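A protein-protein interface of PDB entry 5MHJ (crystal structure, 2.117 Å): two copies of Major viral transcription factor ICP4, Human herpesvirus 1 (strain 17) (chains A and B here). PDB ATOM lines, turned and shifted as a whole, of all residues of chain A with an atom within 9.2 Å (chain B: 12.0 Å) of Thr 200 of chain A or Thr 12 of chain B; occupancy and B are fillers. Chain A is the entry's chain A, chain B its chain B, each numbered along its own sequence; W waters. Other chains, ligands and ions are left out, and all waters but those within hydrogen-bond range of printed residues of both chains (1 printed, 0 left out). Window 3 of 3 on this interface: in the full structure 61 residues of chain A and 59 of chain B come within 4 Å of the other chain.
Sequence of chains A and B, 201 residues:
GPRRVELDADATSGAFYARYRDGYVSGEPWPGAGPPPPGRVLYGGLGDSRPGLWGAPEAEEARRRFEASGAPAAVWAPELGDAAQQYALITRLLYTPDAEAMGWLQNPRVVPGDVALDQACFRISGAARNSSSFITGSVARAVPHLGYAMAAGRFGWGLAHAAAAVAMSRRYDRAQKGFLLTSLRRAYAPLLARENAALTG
The side-chain amide nitrogen (ND2) of Asn 196 of chain A sits at hydrogen-bond distance from the backbone carbonyl oxygen (O) of Ala 11 of chain B (3.0 Å).
The backbone NH (N) of Arg 92 of chain A is in hydrogen-bond range of the side-chain hydroxyl (OH) of Tyr 17 of chain B.
The backbone carbonyl oxygen (O) of Ala 197 of chain A is in hydrogen-bond range of the side-chain hydroxyl (OG1) of Thr 200 of chain A, 3.2 Å away.
OD1 of Asn 196 of chain A lies close to O of Leu 192 of chain A, 3.5 Å away.
NH1 of Arg 154 of chain A lies within hydrogen-bond range of OD1 of Asn 196 of chain A (3.0 Å).
O of Asn 196 of chain A lies within hydrogen-bond range of OG1 of Thr 200 of chain A (2.6 Å).
O of Asp 10 of chain B sits at hydrogen-bond distance from N of Phe 16 of chain B, at 2.9 Å.
The backbone NH (N) of Ala 15 of chain B lies close to the side-chain hydroxyl (OG) of Ser 13 of chain B.
Arg 92 of chain A touches Phe 16 of chain B.
Leu 192 of chain A touches Tyr 17 of chain B (CD1 to CD1, 3.9 Å).
Gly 14 of chain B touches Ala 193 of chain A.
CB of Tyr 17 of chain B touches N of Ala 193 of chain A (3.9 Å).
CB of Ala 193 of chain A touches N of Ala 18 of chain B, 3.5 Å away.
Asn 196 of chain A touches Thr 12 of chain B (CB to O, 3.3 Å).
Gly 14 of chain B touches Asn 196 of chain A (CA to CB, 3.8 Å).
Asn 196 of chain A touches Tyr 17 of chain B.
Ala 197 of chain A touches Ser 13 of chain B.
Thr 200 of chain A touches Thr 12 of chain B.
Leu 89 of chain A touches none of the printed residues of chain B.
Of chain B, only Ala 11 (3.0 Å), Thr 12 (3.3 Å), Gly 14 (3.8 Å) and Tyr 17 (3.8 Å) come within 4 Å of Asn 196 of chain A.
No residue of chain B comes within 4 Å of Ala 198 of chain A.
Printed residues of chain B within 4 Å of Thr 200 of chain A: Thr 12.
Thr 12 of chain B touches just these residues of chain A: Asn 196 (3.3 Å) and Thr 200 (3.9 Å).
Ser 13 of chain B touches just one residue of chain A: Ala 197 (3.6 Å).
Printed residues of chain A within 4 Å of Tyr 17 of chain B: Arg 92 (3.3 Å), Leu 192 (3.9 Å), Ala 193 (3.9 Å) and Asn 196 (3.8 Å).
Printed residues of chain A within 4 Å of Ala 18 of chain B: Ala 193 (3.5 Å).
Arg 19 of chain B touches none of the printed residues of chain A.
The nearest residue of chain B that does not touch Thr 200 of chain A is Ser 13 of chain B (4.7 Å).
Hydrophobic or aromatic side chains of chain B that line the printed part of chain A: Phe 16, Tyr 17 and Ala 18.
Of the 17 printed residues of chain A, 6 touch a printed residue of chain B.
Hydrophobic or aromatic side chains of chain A within 4 Å of the printed part of chain B: Leu 192, Ala 193 and Ala 197.
Among the printed residues, 12 pairs touch across the chains.
No position is printed for both chains.
Of the 12 pairs that touch across the chains among the printed residues, none has its exchanged pair printed and touching as well.
Water W1 lies within hydrogen-bond range of the side-chain hydroxyl of Tyr 17 of chain B (2.5 Å) and the backbone carbonyl oxygen of Ala 88 of chain A (2.8 Å).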
ATOM      1  N   SER A  26       8.620  34.011  12.819  1.00  0.00           N
ATOM      2  CA  SER A  26       9.941  33.759  13.374  1.00  0.00           C
ATOM      3  C   SER A  26      10.832  33.113  12.321  1.00  0.00           C
ATOM      4  O   SER A  26      10.435  32.144  11.667  1.00  0.00           O
ATOM      5  CB  SER A  26       9.834  32.865  14.606  1.00  0.00           C
ATOM      6  OG  SER A  26      11.114  32.457  15.050  1.00  0.00           O
ATOM      7  N   ALA A  84      25.203  34.694  16.532  1.00  0.00           N
ATOM      8  CA  ALA A  84      24.366  33.679  17.162  1.00  0.00           C
ATOM      9  C   ALA A  84      25.065  33.019  18.344  1.00  0.00           C
ATOM     10  O   ALA A  84      24.397  32.598  19.297  1.00  0.00           O
ATOM     11  CB  ALA A  84      23.958  32.623  16.135  1.00  0.00           C
ATOM     12  N   GLN A  85      26.394  32.914  18.306  1.00  0.00           N
ATOM     13  CA  GLN A  85      27.107  32.282  19.412  1.00  0.00           C
ATOM     14  C   GLN A  85      27.130  33.180  20.642  1.00  0.00           C
ATOM     15  O   GLN A  85      26.952  32.702  21.768  1.00  0.00           O
ATOM     16  CB  GLN A  85      28.530  31.917  18.984  1.00  0.00           C
ATOM     17  CG  GLN A  85      29.081  30.681  19.678  1.00  0.00           C
ATOM     18  CD  GLN A  85      30.578  30.756  19.898  1.00  0.00           C
ATOM     19  OE1 GLN A  85      31.216  31.757  19.570  1.00  0.00           O
ATOM     20  NE2 GLN A  85      31.148  29.696  20.460  1.00  0.00           N
ATOM     21  N   ALA A  88      23.651  33.232  22.103  1.00  0.00           N
ATOM     22  CA  ALA A  88      23.367  32.008  22.846  1.00  0.00           C
ATOM     23  C   ALA A  88      24.053  32.012  24.206  1.00  0.00           C
ATOM     24  O   ALA A  88      23.458  31.598  25.209  1.00  0.00           O
ATOM     25  CB  ALA A  88      23.794  30.789  22.028  1.00  0.00           C
ATOM     26  N   LEU A  89      25.300  32.489  24.263  1.00  0.00           N
ATOM     27  CA  LEU A  89      26.025  32.525  25.529  1.00  0.00           C
ATOM     28  C   LEU A  89      25.370  33.478  26.522  1.00  0.00           C
ATOM     29  O   LEU A  89      25.214  33.140  27.702  1.00  0.00           O
ATOM     30  CB  LEU A  89      27.482  32.921  25.285  1.00  0.00           C
ATOM     31  CG  LEU A  89      28.387  31.844  24.678  1.00  0.00           C
ATOM     32  CD1 LEU A  89      29.749  32.424  24.325  1.00  0.00           C
ATOM     33  CD2 LEU A  89      28.533  30.657  25.625  1.00  0.00           C
ATOM     34  N   ARG A  92      21.937  32.136  27.709  1.00  0.00           N
ATOM     35  CA  ARG A  92      22.142  31.086  28.701  1.00  0.00           C
ATOM     36  C   ARG A  92      22.590  31.674  30.033  1.00  0.00           C
ATOM     37  O   ARG A  92      22.090  31.281  31.093  1.00  0.00           O
ATOM     38  CB  ARG A  92      23.162  30.067  28.190  1.00  0.00           C
ATOM     39  CG  ARG A  92      23.371  28.869  29.108  1.00  0.00           C
ATOM     40  CD  ARG A  92      22.079  28.097  29.324  1.00  0.00           C
ATOM     41  NE  ARG A  92      22.310  26.678  29.586  1.00  0.00           N
ATOM     42  CZ  ARG A  92      22.483  26.162  30.800  1.00  0.00           C
ATOM     43  NH1 ARG A  92      22.464  26.951  31.864  1.00  0.00           N
ATOM     44  NH2 ARG A  92      22.682  24.859  30.951  1.00  0.00           N
ATOM     45  N   ARG A 154      14.820  36.655  14.981  1.00  0.00           N
ATOM     46  CA  ARG A 154      14.963  35.923  16.238  1.00  0.00           C
ATOM     47  C   ARG A 154      14.425  36.806  17.358  1.00  0.00           C
ATOM     48  O   ARG A 154      15.154  37.597  17.958  1.00  0.00           O
ATOM     49  CB  ARG A 154      16.417  35.530  16.479  1.00  0.00           C
ATOM     50  CG  ARG A 154      16.850  34.259  15.764  1.00  0.00           C
ATOM     51  CD  ARG A 154      17.121  33.137  16.758  1.00  0.00           C
ATOM     52  NE  ARG A 154      17.704  31.962  16.119  1.00  0.00           N
ATOM     53  CZ  ARG A 154      18.087  30.869  16.772  1.00  0.00           C
ATOM     54  NH1 ARG A 154      17.949  30.800  18.088  1.00  0.00           N
ATOM     55  NH2 ARG A 154      18.608  29.845  16.109  1.00  0.00           N
ATOM     56  N   TRP A 157      16.100  36.651  20.860  1.00  0.00           N
ATOM     57  CA  TRP A 157      17.304  37.436  21.098  1.00  0.00           C
ATOM     58  C   TRP A 157      17.000  38.833  21.623  1.00  0.00           C
ATOM     59  O   TRP A 157      17.933  39.564  21.969  1.00  0.00           O
ATOM     60  CB  TRP A 157      18.131  37.535  19.810  1.00  0.00           C
ATOM     61  CG  TRP A 157      18.798  36.241  19.431  1.00  0.00           C
ATOM     62  CD1 TRP A 157      18.850  35.100  20.176  1.00  0.00           C
ATOM     63  CD2 TRP A 157      19.506  35.958  18.215  1.00  0.00           C
ATOM     64  NE1 TRP A 157      19.543  34.125  19.504  1.00  0.00           N
ATOM     65  CE2 TRP A 157      19.956  34.625  18.298  1.00  0.00           C
ATOM     66  CE3 TRP A 157      19.800  36.700  17.066  1.00  0.00           C
ATOM     67  CZ2 TRP A 157      20.688  34.018  17.277  1.00  0.00           C
ATOM     68  CZ3 TRP A 157      20.528  36.096  16.052  1.00  0.00           C
ATOM     69  CH2 TRP A 157      20.962  34.768  16.165  1.00  0.00           C
ATOM     70  N   LEU A 192      11.817  31.153  23.929  1.00  0.00           N
ATOM     71  CA  LEU A 192      13.125  30.656  23.519  1.00  0.00           C
ATOM     72  C   LEU A 192      13.075  29.165  23.206  1.00  0.00           C
ATOM     73  O   LEU A 192      13.687  28.707  22.235  1.00  0.00           O
ATOM     74  CB  LEU A 192      14.158  30.944  24.609  1.00  0.00           C
ATOM     75  CG  LEU A 192      14.525  32.413  24.831  1.00  0.00           C
ATOM     76  CD1 LEU A 192      15.109  32.605  26.222  1.00  0.00           C
ATOM     77  CD2 LEU A 192      15.503  32.887  23.769  1.00  0.00           C
ATOM     78  N   ALA A 193      12.346  28.393  24.017  1.00  0.00           N
ATOM     79  CA  ALA A 193      12.222  26.962  23.763  1.00  0.00           C
ATOM     80  C   ALA A 193      11.546  26.694  22.424  1.00  0.00           C
ATOM     81  O   ALA A 193      11.964  25.805  21.674  1.00  0.00           O
ATOM     82  CB  ALA A 193      11.444  26.293  24.896  1.00  0.00           C
ATOM     83  N   ARG A 194      10.493  27.451  22.111  1.00  0.00           N
ATOM     84  CA  ARG A 194       9.795  27.260  20.845  1.00  0.00           C
ATOM     85  C   ARG A 194      10.632  27.750  19.671  1.00  0.00           C
ATOM     86  O   ARG A 194      10.699  27.089  18.626  1.00  0.00           O
ATOM     87  CB  ARG A 194       8.447  27.979  20.886  1.00  0.00           C
ATOM     88  CG  ARG A 194       7.550  27.724  19.689  1.00  0.00           C
ATOM     89  CD  ARG A 194       6.242  28.499  19.811  1.00  0.00           C
ATOM     90  NE  ARG A 194       5.749  28.542  21.187  1.00  0.00           N
ATOM     91  CZ  ARG A 194       5.517  29.663  21.864  1.00  0.00           C
ATOM     92  NH1 ARG A 194       5.732  30.842  21.295  1.00  0.00           N
ATOM     93  NH2 ARG A 194       5.070  29.608  23.111  1.00  0.00           N
ATOM     94  N   GLU A 195      11.289  28.900  19.826  1.00  0.00           N
ATOM     95  CA  GLU A 195      12.062  29.468  18.726  1.00  0.00           C
ATOM     96  C   GLU A 195      13.300  28.631  18.426  1.00  0.00           C
ATOM     97  O   GLU A 195      13.638  28.410  17.258  1.00  0.00           O
ATOM     98  CB  GLU A 195      12.441  30.912  19.054  1.00  0.00           C
ATOM     99  CG  GLU A 195      13.057  31.692  17.905  1.00  0.00           C
ATOM    100  CD  GLU A 195      12.874  33.189  18.071  1.00  0.00           C
ATOM    101  OE1 GLU A 195      11.874  33.738  17.557  1.00  0.00           O
ATOM    102  OE2 GLU A 195      13.721  33.816  18.741  1.00  0.00           O
ATOM    103  N   ASN A 196      13.987  28.148  19.465  1.00  0.00           N
ATOM    104  CA  ASN A 196      15.188  27.349  19.244  1.00  0.00           C
ATOM    105  C   ASN A 196      14.850  26.006  18.610  1.00  0.00           C
ATOM    106  O   ASN A 196      15.586  25.518  17.745  1.00  0.00           O
ATOM    107  CB  ASN A 196      15.939  27.149  20.559  1.00  0.00           C
ATOM    108  CG  ASN A 196      16.659  28.402  21.016  1.00  0.00           C
ATOM    109  OD1 ASN A 196      16.549  29.461  20.395  1.00  0.00           O
ATOM    110  ND2 ASN A 196      17.400  28.290  22.111  1.00  0.00           N
ATOM    111  N   ALA A 197      13.737  25.394  19.023  1.00  0.00           N
ATOM    112  CA  ALA A 197      13.342  24.110  18.451  1.00  0.00           C
ATOM    113  C   ALA A 197      12.978  24.242  16.976  1.00  0.00           C
ATOM    114  O   ALA A 197      13.261  23.339  16.181  1.00  0.00           O
ATOM    115  CB  ALA A 197      12.172  23.521  19.241  1.00  0.00           C
ATOM    116  N   ALA A 198      12.353  25.357  16.592  1.00  0.00           N
ATOM    117  CA  ALA A 198      11.916  25.524  15.209  1.00  0.00           C
ATOM    118  C   ALA A 198      13.080  25.865  14.287  1.00  0.00           C
ATOM    119  O   ALA A 198      13.218  25.271  13.212  1.00  0.00           O
ATOM    120  CB  ALA A 198      10.829  26.598  15.130  1.00  0.00           C
ATOM    121  N   LEU A 199      13.936  26.804  14.699  1.00  0.00           N
ATOM    122  CA  LEU A 199      15.059  27.272  13.891  1.00  0.00           C
ATOM    123  C   LEU A 199      16.274  26.346  13.960  1.00  0.00           C
ATOM    124  O   LEU A 199      17.404  26.806  13.773  1.00  0.00           O
ATOM    125  CB  LEU A 199      15.441  28.695  14.309  1.00  0.00           C
ATOM    126  CG  LEU A 199      14.314  29.728  14.181  1.00  0.00           C
ATOM    127  CD1 LEU A 199      14.768  31.106  14.639  1.00  0.00           C
ATOM    128  CD2 LEU A 199      13.770  29.778  12.756  1.00  0.00           C
ATOM    129  N   THR A 200      16.063  25.060  14.226  1.00  0.00           N
ATOM    130  CA  THR A 200      17.153  24.083  14.225  1.00  0.00           C
ATOM    131  C   THR A 200      16.726  22.798  13.530  1.00  0.00           C
ATOM    132  O   THR A 200      15.565  22.399  13.606  1.00  0.00           O
ATOM    133  CB  THR A 200      17.617  23.737  15.652  1.00  0.00           C
ATOM    134  OG1 THR A 200      16.481  23.455  16.476  1.00  0.00           O
ATOM    135  CG2 THR A 200      18.414  24.882  16.263  1.00  0.00           C
ATOM    136  N   ASP B   8      26.552  21.790  24.142  1.00  0.00           N
ATOM    137  CA  ASP B   8      25.512  22.728  24.545  1.00  0.00           C
ATOM    138  C   ASP B   8      24.224  22.489  23.760  1.00  0.00           C
ATOM    139  O   ASP B   8      23.464  23.421  23.491  1.00  0.00           O
ATOM    140  CB  ASP B   8      25.990  24.169  24.355  1.00  0.00           C
ATOM    141  CG  ASP B   8      25.785  25.017  25.594  1.00  0.00           C
ATOM    142  OD1 ASP B   8      24.856  24.717  26.375  1.00  0.00           O
ATOM    143  OD2 ASP B   8      26.553  25.983  25.789  1.00  0.00           O
ATOM    144  N   ALA B   9      23.983  21.226  23.399  1.00  0.00           N
ATOM    145  CA  ALA B   9      22.794  20.885  22.629  1.00  0.00           C
ATOM    146  C   ALA B   9      21.512  21.051  23.433  1.00  0.00           C
ATOM    147  O   ALA B   9      20.440  21.200  22.838  1.00  0.00           O
ATOM    148  CB  ALA B   9      22.901  19.450  22.109  1.00  0.00           C
ATOM    149  N   ASP B  10      21.598  21.031  24.765  1.00  0.00           N
ATOM    150  CA  ASP B  10      20.405  21.191  25.590  1.00  0.00           C
ATOM    151  C   ASP B  10      19.810  22.586  25.433  1.00  0.00           C
ATOM    152  O   ASP B  10      18.584  22.743  25.380  1.00  0.00           O
ATOM    153  CB  ASP B  10      20.745  20.910  27.054  1.00  0.00           C
ATOM    154  CG  ASP B  10      19.513  20.693  27.909  1.00  0.00           C
ATOM    155  OD1 ASP B  10      18.655  19.876  27.515  1.00  0.00           O
ATOM    156  OD2 ASP B  10      19.407  21.330  28.978  1.00  0.00           O
ATOM    157  N   ALA B  11      20.661  23.609  25.351  1.00  0.00           N
ATOM    158  CA  ALA B  11      20.184  24.974  25.173  1.00  0.00           C
ATOM    159  C   ALA B  11      19.892  25.294  23.712  1.00  0.00           C
ATOM    160  O   ALA B  11      18.951  26.041  23.422  1.00  0.00           O
ATOM    161  CB  ALA B  11      21.207  25.964  25.734  1.00  0.00           C
ATOM    162  N   THR B  12      20.678  24.742  22.784  1.00  0.00           N
ATOM    163  CA  THR B  12      20.456  25.012  21.368  1.00  0.00           C
ATOM    164  C   THR B  12      19.136  24.418  20.891  1.00  0.00           C
ATOM    165  O   THR B  12      18.394  25.059  20.139  1.00  0.00           O
ATOM    166  CB  THR B  12      21.628  24.471  20.547  1.00  0.00           C
ATOM    167  OG1 THR B  12      22.789  25.274  20.795  1.00  0.00           O
ATOM    168  CG2 THR B  12      21.309  24.494  19.059  1.00  0.00           C
ATOM    169  N   SER B  13      18.818  23.197  21.326  1.00  0.00           N
ATOM    170  CA  SER B  13      17.556  22.576  20.948  1.00  0.00           C
ATOM    171  C   SER B  13      16.356  23.205  21.641  1.00  0.00           C
ATOM    172  O   SER B  13      15.219  22.909  21.260  1.00  0.00           O
ATOM    173  CB  SER B  13      17.595  21.079  21.255  1.00  0.00           C
ATOM    174  OG  SER B  13      17.571  20.852  22.655  1.00  0.00           O
ATOM    175  N   GLY B  14      16.578  24.056  22.642  1.00  0.00           N
ATOM    176  CA  GLY B  14      15.498  24.679  23.376  1.00  0.00           C
ATOM    177  C   GLY B  14      14.996  23.895  24.565  1.00  0.00           C
ATOM    178  O   GLY B  14      14.164  24.415  25.319  1.00  0.00           O
ATOM    179  N   ALA B  15      15.477  22.665  24.767  1.00  0.00           N
ATOM    180  CA  ALA B  15      14.981  21.847  25.867  1.00  0.00           C
ATOM    181  C   ALA B  15      15.301  22.466  27.220  1.00  0.00           C
ATOM    182  O   ALA B  15      14.512  22.336  28.162  1.00  0.00           O
ATOM    183  CB  ALA B  15      15.562  20.436  25.777  1.00  0.00           C
ATOM    184  N   PHE B  16      16.446  23.145  27.337  1.00  0.00           N
ATOM    185  CA  PHE B  16      16.795  23.785  28.602  1.00  0.00           C
ATOM    186  C   PHE B  16      15.777  24.853  28.978  1.00  0.00           C
ATOM    187  O   PHE B  16      15.357  24.941  30.137  1.00  0.00           O
ATOM    188  CB  PHE B  16      18.195  24.392  28.522  1.00  0.00           C
ATOM    189  CG  PHE B  16      18.550  25.252  29.704  1.00  0.00           C
ATOM    190  CD1 PHE B  16      18.967  24.678  30.894  1.00  0.00           C
ATOM    191  CD2 PHE B  16      18.467  26.635  29.627  1.00  0.00           C
ATOM    192  CE1 PHE B  16      19.294  25.463  31.985  1.00  0.00           C
ATOM    193  CE2 PHE B  16      18.792  27.426  30.715  1.00  0.00           C
ATOM    194  CZ  PHE B  16      19.206  26.837  31.896  1.00  0.00           C
ATOM    195  N   TYR B  17      15.369  25.679  28.013  1.00  0.00           N
ATOM    196  CA  TYR B  17      14.448  26.761  28.331  1.00  0.00           C
ATOM    197  C   TYR B  17      13.037  26.241  28.575  1.00  0.00           C
ATOM    198  O   TYR B  17      12.285  26.839  29.353  1.00  0.00           O
ATOM    199  CB  TYR B  17      14.480  27.808  27.218  1.00  0.00           C
ATOM    200  CG  TYR B  17      15.857  28.402  27.045  1.00  0.00           C
ATOM    201  CD1 TYR B  17      16.340  29.346  27.940  1.00  0.00           C
ATOM    202  CD2 TYR B  17      16.690  27.995  26.008  1.00  0.00           C
ATOM    203  CE1 TYR B  17      17.604  29.883  27.804  1.00  0.00           C
ATOM    204  CE2 TYR B  17      17.960  28.528  25.862  1.00  0.00           C
ATOM    205  CZ  TYR B  17      18.409  29.473  26.764  1.00  0.00           C
ATOM    206  OH  TYR B  17      19.666  30.017  26.639  1.00  0.00           O
ATOM    207  N   ALA B  18      12.669  25.122  27.948  1.00  0.00           N
ATOM    208  CA  ALA B  18      11.369  24.517  28.213  1.00  0.00           C
ATOM    209  C   ALA B  18      11.284  23.919  29.611  1.00  0.00           C
ATOM    210  O   ALA B  18      10.177  23.740  30.130  1.00  0.00           O
ATOM    211  CB  ALA B  18      11.067  23.441  27.167  1.00  0.00           C
ATOM    212  N   ARG B  19      12.424  23.616  30.232  1.00  0.00           N
ATOM    213  CA  ARG B  19      12.462  23.026  31.562  1.00  0.00           C
ATOM    214  C   ARG B  19      12.632  24.050  32.674  1.00  0.00           C
ATOM    215  O   ARG B  19      12.415  23.707  33.842  1.00  0.00           O
ATOM    216  CB  ARG B  19      13.601  22.000  31.661  1.00  0.00           C
ATOM    217  CG  ARG B  19      13.415  20.753  30.813  1.00  0.00           C
ATOM    218  CD  ARG B  19      14.351  19.645  31.270  1.00  0.00           C
ATOM    219  NE  ARG B  19      15.647  20.172  31.690  1.00  0.00           N
ATOM    220  CZ  ARG B  19      16.681  20.354  30.875  1.00  0.00           C
ATOM    221  NH1 ARG B  19      16.579  20.048  29.587  1.00  0.00           N
ATOM    222  NH2 ARG B  19      17.819  20.844  31.346  1.00  0.00           N
HETATM  223  O   HOH W   1      21.457  29.708  24.869  1.00  0.00           O
